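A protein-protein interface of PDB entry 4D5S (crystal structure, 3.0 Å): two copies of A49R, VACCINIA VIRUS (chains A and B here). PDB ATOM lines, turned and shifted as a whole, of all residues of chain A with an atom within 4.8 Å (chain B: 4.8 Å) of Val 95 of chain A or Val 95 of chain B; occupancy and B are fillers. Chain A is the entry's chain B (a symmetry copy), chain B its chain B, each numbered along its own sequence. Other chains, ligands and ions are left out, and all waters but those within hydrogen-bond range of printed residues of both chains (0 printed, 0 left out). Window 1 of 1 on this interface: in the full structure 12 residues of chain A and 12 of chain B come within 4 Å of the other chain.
NE of Arg 136 of chain A lies within salt-bridge range of OD1 of Asp 92 of chain B (3.6 Å). The guanidinium group of Arg 136 of chain B is in salt-bridge range of the side-chain carboxylate of Asp 92 of chain A (3.6 Å). The side-chain sulfur of Met 99 of chain A lies close to the side-chain sulfur of Met 99 of chain B, 3.5 Å away.
Printed residues of chain A that touch a printed residue of chain B: Asp 92, Val 95, Asn 96, Phe 98, Met 99 and Arg 136. Among the printed residues, 10 pairs touch across the chains. Among the printed residues, Asp or Glu carboxylates within 4 Å of a Lys or Arg side-chain nitrogen of the other chain: Asp 92 of chain A with Arg 136 of chain B (3.6 Å) and Arg 136 of chain A with Asp 92 of chain B (3.6 Å).
Asp 92 of chain A touches Arg 136 of chain B, and with the chains exchanged Arg 136 of chain A touches Asp 92 of chain B. Asn 96 of chain A touches Arg 136 of chain B, and with the chains exchanged Arg 136 of chain A touches Asn 96 of chain B. Phe 98 of chain A touches Met 99 of chain B, and with the chains exchanged Met 99 of chain A touches Phe 98 of chain B. Met 99 of chain B touches its own counterpart, Met 99 of chain A. Of the 10 pairs that touch across the chains among the printed residues, 10 have their exchanged pair printed and touching as well.
Of chain B, only Val 95 and Arg 136 come within 4 Å of Val 95 of chain A. Val 95 of chain B touches two residues of chain A. Printed residues of chain A within 4 Å of Phe 98 of chain B: Met 99 (3.5 Å). Of the printed residues of chain B, Met 99 of chain A touches Phe 98 (3.5 Å) and Met 99 (3.5 Å). Printed residues of chain A within 4 Å of Asn 96 of chain B: Arg 136. Of the printed residues of chain A, Arg 136 of chain B touches Asp 92 (3.6 Å), Val 95 (3.9 Å) and Asn 96 (3.8 Å). Of the printed residues of chain B, Asp 92 of chain A touches Arg 136 (3.6 Å). CSO 93 of chain B touches none of the printed residues of chain A. The nearest residue of chain A that does not touch Val 95 of chain B is Phe 98 of chain A (4.6 Å).
Val 95 of chain A touches Val 95 of chain B. CD of Arg 136 of chain B touches CG1 of Val 95 of chain A, at 3.9 Å. NE of Arg 136 of chain B touches CB of Asn 96 of chain A, at 3.8 Å. Phe 98 of chain A touches Met 99 of chain B (CD1 to CE, 3.5 Å). CE of Met 99 of chain A touches CD1 of Phe 98 of chain B (3.5 Å). CD of Arg 136 of chain A touches CG1 of Val 95 of chain B, at 3.9 Å. NE of Arg 136 of chain A touches CB of Asn 96 of chain B (3.8 Å).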
ATOM      1  N   ILE A  91     -17.254 -22.988  -3.604  1.00  0.00           N
ATOM      2  CA  ILE A  91     -17.919 -24.197  -3.143  1.00  0.00           C
ATOM      3  C   ILE A  91     -18.146 -24.127  -1.625  1.00  0.00           C
ATOM      4  O   ILE A  91     -19.264 -24.329  -1.138  1.00  0.00           O
ATOM      5  CB  ILE A  91     -17.103 -25.442  -3.573  1.00  0.00           C
ATOM      6  CG1 ILE A  91     -17.082 -25.552  -5.115  1.00  0.00           C
ATOM      7  CG2 ILE A  91     -17.682 -26.711  -2.959  1.00  0.00           C
ATOM      8  CD1 ILE A  91     -15.877 -26.275  -5.684  1.00  0.00           C
ATOM      9  N   ASP A  92     -17.091 -23.791  -0.888  1.00  0.00           N
ATOM     10  CA  ASP A  92     -17.224 -23.576   0.543  1.00  0.00           C
ATOM     11  C   ASP A  92     -18.340 -22.576   0.826  1.00  0.00           C
ATOM     12  O   ASP A  92     -19.202 -22.842   1.668  1.00  0.00           O
ATOM     13  CB  ASP A  92     -15.905 -23.100   1.141  1.00  0.00           C
ATOM     14  CG  ASP A  92     -15.836 -23.354   2.618  1.00  0.00           C
ATOM     15  OD1 ASP A  92     -16.601 -22.716   3.355  1.00  0.00           O
ATOM     16  OD2 ASP A  92     -15.040 -24.214   3.044  1.00  0.00           O
ATOM     17  N   CSO A  93     -18.334 -21.447   0.099  1.00  0.00           N
ATOM     18  CA  CSO A  93     -19.339 -20.376   0.293  1.00  0.00           C
ATOM     19  CB  CSO A  93     -19.191 -19.144  -0.621  1.00  0.00           C
ATOM     20  SG  CSO A  93     -20.283 -17.847  -0.112  1.00  0.00           S
ATOM     21  C   CSO A  93     -20.663 -21.000   0.085  1.00  0.00           C
ATOM     22  O   CSO A  93     -21.507 -21.018   0.961  1.00  0.00           O
ATOM     23  OD  CSO A  93     -19.254 -16.500   0.317  1.00  0.00           O
ATOM     24  N   ILE A  94     -20.842 -21.585  -1.072  1.00  0.00           N
ATOM     25  CA  ILE A  94     -22.131 -22.160  -1.396  1.00  0.00           C
ATOM     26  C   ILE A  94     -22.653 -23.114  -0.322  1.00  0.00           C
ATOM     27  O   ILE A  94     -23.777 -22.980   0.166  1.00  0.00           O
ATOM     28  CB  ILE A  94     -22.065 -22.905  -2.727  1.00  0.00           C
ATOM     29  CG1 ILE A  94     -21.913 -21.892  -3.863  1.00  0.00           C
ATOM     30  CG2 ILE A  94     -23.332 -23.724  -2.914  1.00  0.00           C
ATOM     31  CD1 ILE A  94     -21.644 -22.491  -5.220  1.00  0.00           C
ATOM     32  N   VAL A  95     -21.835 -24.087   0.041  1.00  0.00           N
ATOM     33  CA  VAL A  95     -22.304 -25.102   0.955  1.00  0.00           C
ATOM     34  C   VAL A  95     -22.565 -24.473   2.316  1.00  0.00           C
ATOM     35  O   VAL A  95     -23.527 -24.813   2.975  1.00  0.00           O
ATOM     36  CB  VAL A  95     -21.301 -26.254   1.075  1.00  0.00           C
ATOM     37  CG1 VAL A  95     -21.762 -27.262   2.110  1.00  0.00           C
ATOM     38  CG2 VAL A  95     -21.117 -26.951  -0.262  1.00  0.00           C
ATOM     39  N   ASN A  96     -21.713 -23.545   2.730  1.00  0.00           N
ATOM     40  CA  ASN A  96     -21.892 -22.903   4.021  1.00  0.00           C
ATOM     41  C   ASN A  96     -23.215 -22.159   4.087  1.00  0.00           C
ATOM     42  O   ASN A  96     -23.968 -22.315   5.034  1.00  0.00           O
ATOM     43  CB  ASN A  96     -20.738 -21.936   4.297  1.00  0.00           C
ATOM     44  CG  ASN A  96     -21.029 -21.000   5.453  1.00  0.00           C
ATOM     45  OD1 ASN A  96     -21.765 -21.365   6.372  1.00  0.00           O
ATOM     46  ND2 ASN A  96     -20.447 -19.794   5.425  1.00  0.00           N
ATOM     47  N   LYS A  97     -23.473 -21.347   3.071  1.00  0.00           N
ATOM     48  CA  LYS A  97     -24.651 -20.501   3.032  1.00  0.00           C
ATOM     49  C   LYS A  97     -25.913 -21.340   2.989  1.00  0.00           C
ATOM     50  O   LYS A  97     -26.936 -21.045   3.622  1.00  0.00           O
ATOM     51  CB  LYS A  97     -24.628 -19.606   1.776  1.00  0.00           C
ATOM     52  CG  LYS A  97     -23.474 -18.607   1.680  1.00  0.00           C
ATOM     53  CD  LYS A  97     -23.598 -17.497   2.695  1.00  0.00           C
ATOM     54  CE  LYS A  97     -22.238 -16.950   3.040  1.00  0.00           C
ATOM     55  NZ  LYS A  97     -22.430 -15.776   3.927  1.00  0.00           N
ATOM     56  N   PHE A  98     -25.852 -22.399   2.216  1.00  0.00           N
ATOM     57  CA  PHE A  98     -27.049 -23.151   1.941  1.00  0.00           C
ATOM     58  C   PHE A  98     -27.613 -23.775   3.209  1.00  0.00           C
ATOM     59  O   PHE A  98     -28.799 -24.034   3.323  1.00  0.00           O
ATOM     60  CB  PHE A  98     -26.732 -24.215   0.919  1.00  0.00           C
ATOM     61  CG  PHE A  98     -27.805 -24.398  -0.090  1.00  0.00           C
ATOM     62  CD1 PHE A  98     -28.876 -25.192   0.204  1.00  0.00           C
ATOM     63  CD2 PHE A  98     -27.736 -23.803  -1.331  1.00  0.00           C
ATOM     64  CE1 PHE A  98     -29.886 -25.407  -0.731  1.00  0.00           C
ATOM     65  CE2 PHE A  98     -28.726 -24.003  -2.270  1.00  0.00           C
ATOM     66  CZ  PHE A  98     -29.813 -24.814  -1.977  1.00  0.00           C
ATOM     67  N   MET A  99     -26.757 -23.979   4.185  1.00  0.00           N
ATOM     68  CA  MET A  99     -27.186 -24.560   5.426  1.00  0.00           C
ATOM     69  C   MET A  99     -28.204 -23.718   6.154  1.00  0.00           C
ATOM     70  O   MET A  99     -28.975 -24.248   6.934  1.00  0.00           O
ATOM     71  CB  MET A  99     -25.963 -24.820   6.297  1.00  0.00           C
ATOM     72  CG  MET A  99     -25.001 -25.838   5.667  1.00  0.00           C
ATOM     73  SD  MET A  99     -25.838 -27.219   4.804  1.00  0.00           S
ATOM     74  CE  MET A  99     -24.582 -27.693   3.638  1.00  0.00           C
ATOM     75  N   ARG A 136     -31.212 -27.684  -5.891  1.00  0.00           N
ATOM     76  CA  ARG A 136     -31.149 -27.838  -4.446  1.00  0.00           C
ATOM     77  C   ARG A 136     -32.117 -26.930  -3.722  1.00  0.00           C
ATOM     78  O   ARG A 136     -32.588 -27.244  -2.615  1.00  0.00           O
ATOM     79  CB  ARG A 136     -29.739 -27.594  -3.940  1.00  0.00           C
ATOM     80  CG  ARG A 136     -28.700 -28.533  -4.513  1.00  0.00           C
ATOM     81  CD  ARG A 136     -28.733 -29.926  -3.916  1.00  0.00           C
ATOM     82  NE  ARG A 136     -29.572 -30.855  -4.652  1.00  0.00           N
ATOM     83  CZ  ARG A 136     -30.777 -31.258  -4.265  1.00  0.00           C
ATOM     84  NH1 ARG A 136     -31.325 -30.808  -3.126  1.00  0.00           N
ATOM     85  NH2 ARG A 136     -31.443 -32.121  -5.028  1.00  0.00           N
ATOM     86  N   ILE B  91     -20.487 -32.151  -6.911  1.00  0.00           N
ATOM     87  CA  ILE B  91     -20.930 -30.990  -6.153  1.00  0.00           C
ATOM     88  C   ILE B  91     -22.416 -31.136  -5.789  1.00  0.00           C
ATOM     89  O   ILE B  91     -22.802 -30.999  -4.623  1.00  0.00           O
ATOM     90  CB  ILE B  91     -20.630 -29.696  -6.951  1.00  0.00           C
ATOM     91  CG1 ILE B  91     -19.102 -29.519  -7.111  1.00  0.00           C
ATOM     92  CG2 ILE B  91     -21.235 -28.479  -6.262  1.00  0.00           C
ATOM     93  CD1 ILE B  91     -18.679 -28.724  -8.331  1.00  0.00           C
ATOM     94  N   ASP B  92     -23.236 -31.461  -6.784  1.00  0.00           N
ATOM     95  CA  ASP B  92     -24.638 -31.743  -6.528  1.00  0.00           C
ATOM     96  C   ASP B  92     -24.774 -32.798  -5.434  1.00  0.00           C
ATOM     97  O   ASP B  92     -25.540 -32.603  -4.486  1.00  0.00           O
ATOM     98  CB  ASP B  92     -25.340 -32.192  -7.804  1.00  0.00           C
ATOM     99  CG  ASP B  92     -26.825 -32.000  -7.724  1.00  0.00           C
ATOM    100  OD1 ASP B  92     -27.460 -32.699  -6.921  1.00  0.00           O
ATOM    101  OD2 ASP B  92     -27.359 -31.129  -8.439  1.00  0.00           O
ATOM    102  N   CSO B  93     -24.006 -33.894  -5.558  1.00  0.00           N
ATOM    103  CA  CSO B  93     -24.062 -35.011  -4.587  1.00  0.00           C
ATOM    104  CB  CSO B  93     -23.118 -36.195  -4.873  1.00  0.00           C
ATOM    105  SG  CSO B  93     -23.469 -37.555  -3.796  1.00  0.00           S
ATOM    106  C   CSO B  93     -23.753 -34.431  -3.261  1.00  0.00           C
ATOM    107  O   CSO B  93     -24.546 -34.485  -2.339  1.00  0.00           O
ATOM    108  OD  CSO B  93     -23.940 -38.878  -4.838  1.00  0.00           O
ATOM    109  N   ILE B  94     -22.608 -33.804  -3.166  1.00  0.00           N
ATOM    110  CA  ILE B  94     -22.187 -33.267  -1.890  1.00  0.00           C
ATOM    111  C   ILE B  94     -23.243 -32.382  -1.228  1.00  0.00           C
ATOM    112  O   ILE B  94     -23.617 -32.582  -0.071  1.00  0.00           O
ATOM    113  CB  ILE B  94     -20.899 -32.462  -2.047  1.00  0.00           C
ATOM    114  CG1 ILE B  94     -19.743 -33.418  -2.349  1.00  0.00           C
ATOM    115  CG2 ILE B  94     -20.624 -31.687  -0.768  1.00  0.00           C
ATOM    116  CD1 ILE B  94     -18.443 -32.751  -2.716  1.00  0.00           C
ATOM    117  N   VAL B  95     -23.720 -31.394  -1.965  1.00  0.00           N
ATOM    118  CA  VAL B  95     -24.625 -30.439  -1.369  1.00  0.00           C
ATOM    119  C   VAL B  95     -25.929 -31.137  -1.010  1.00  0.00           C
ATOM    120  O   VAL B  95     -26.507 -30.864   0.023  1.00  0.00           O
ATOM    121  CB  VAL B  95     -24.886 -29.255  -2.305  1.00  0.00           C
ATOM    122  CG1 VAL B  95     -25.911 -28.312  -1.707  1.00  0.00           C
ATOM    123  CG2 VAL B  95     -23.601 -28.494  -2.583  1.00  0.00           C
ATOM    124  N   ASN B  96     -26.385 -32.048  -1.860  1.00  0.00           N
ATOM    125  CA  ASN B  96     -27.627 -32.751  -1.589  1.00  0.00           C
ATOM    126  C   ASN B  96     -27.537 -33.550  -0.299  1.00  0.00           C
ATOM    127  O   ASN B  96     -28.414 -33.465   0.546  1.00  0.00           O
ATOM    128  CB  ASN B  96     -27.973 -33.683  -2.753  1.00  0.00           C
ATOM    129  CG  ASN B  96     -29.058 -34.680  -2.396  1.00  0.00           C
ATOM    130  OD1 ASN B  96     -29.917 -34.384  -1.563  1.00  0.00           O
ATOM    131  ND2 ASN B  96     -29.038 -35.859  -3.031  1.00  0.00           N
ATOM    132  N   LYS B  97     -26.470 -34.326  -0.173  1.00  0.00           N
ATOM    133  CA  LYS B  97     -26.286 -35.215   0.958  1.00  0.00           C
ATOM    134  C   LYS B  97     -26.156 -34.426   2.247  1.00  0.00           C
ATOM    135  O   LYS B  97     -26.677 -34.789   3.310  1.00  0.00           O
ATOM    136  CB  LYS B  97     -25.003 -36.054   0.779  1.00  0.00           C
ATOM    137  CG  LYS B  97     -24.978 -37.001  -0.421  1.00  0.00           C
ATOM    138  CD  LYS B  97     -25.932 -38.158  -0.251  1.00  0.00           C
ATOM    139  CE  LYS B  97     -26.383 -38.665  -1.596  1.00  0.00           C
ATOM    140  NZ  LYS B  97     -27.200 -39.884  -1.373  1.00  0.00           N
ATOM    141  N   PHE B  98     -25.435 -33.333   2.160  1.00  0.00           N
ATOM    142  CA  PHE B  98     -25.077 -32.618   3.358  1.00  0.00           C
ATOM    143  C   PHE B  98     -26.309 -32.073   4.064  1.00  0.00           C
ATOM    144  O   PHE B  98     -26.321 -31.866   5.266  1.00  0.00           O
ATOM    145  CB  PHE B  98     -24.133 -31.499   2.993  1.00  0.00           C
ATOM    146  CG  PHE B  98     -23.035 -31.314   3.974  1.00  0.00           C
ATOM    147  CD1 PHE B  98     -23.257 -30.577   5.101  1.00  0.00           C
ATOM    148  CD2 PHE B  98     -21.783 -31.851   3.763  1.00  0.00           C
ATOM    149  CE1 PHE B  98     -22.239 -30.361   6.028  1.00  0.00           C
ATOM    150  CE2 PHE B  98     -20.763 -31.650   4.669  1.00  0.00           C
ATOM    151  CZ  PHE B  98     -20.983 -30.896   5.813  1.00  0.00           C
ATOM    152  N   MET B  99     -27.370 -31.877   3.313  1.00  0.00           N
ATOM    153  CA  MET B  99     -28.586 -31.369   3.881  1.00  0.00           C
ATOM    154  C   MET B  99     -29.180 -32.281   4.924  1.00  0.00           C
ATOM    155  O   MET B  99     -29.904 -31.816   5.787  1.00  0.00           O
ATOM    156  CB  MET B  99     -29.580 -31.098   2.757  1.00  0.00           C
ATOM    157  CG  MET B  99     -29.085 -30.016   1.785  1.00  0.00           C
ATOM    158  SD  MET B  99     -28.202 -28.634   2.597  1.00  0.00           S
ATOM    159  CE  MET B  99     -27.180 -28.059   1.260  1.00  0.00           C
ATOM    160  N   ARG B 136     -17.070 -27.916   6.964  1.00  0.00           N
ATOM    161  CA  ARG B 136     -18.520 -27.823   7.043  1.00  0.00           C
ATOM    162  C   ARG B 136     -19.112 -28.800   8.034  1.00  0.00           C
ATOM    163  O   ARG B 136     -20.181 -28.553   8.620  1.00  0.00           O
ATOM    164  CB  ARG B 136     -19.148 -28.033   5.677  1.00  0.00           C
ATOM    165  CG  ARG B 136     -18.714 -27.030   4.631  1.00  0.00           C
ATOM    166  CD  ARG B 136     -19.360 -25.666   4.780  1.00  0.00           C
ATOM    167  NE  ARG B 136     -18.584 -24.740   5.586  1.00  0.00           N
ATOM    168  CZ  ARG B 136     -18.871 -24.403   6.839  1.00  0.00           C
ATOM    169  NH1 ARG B 136     -19.934 -24.922   7.471  1.00  0.00           N
ATOM    170  NH2 ARG B 136     -18.083 -23.534   7.468  1.00  0.00           N
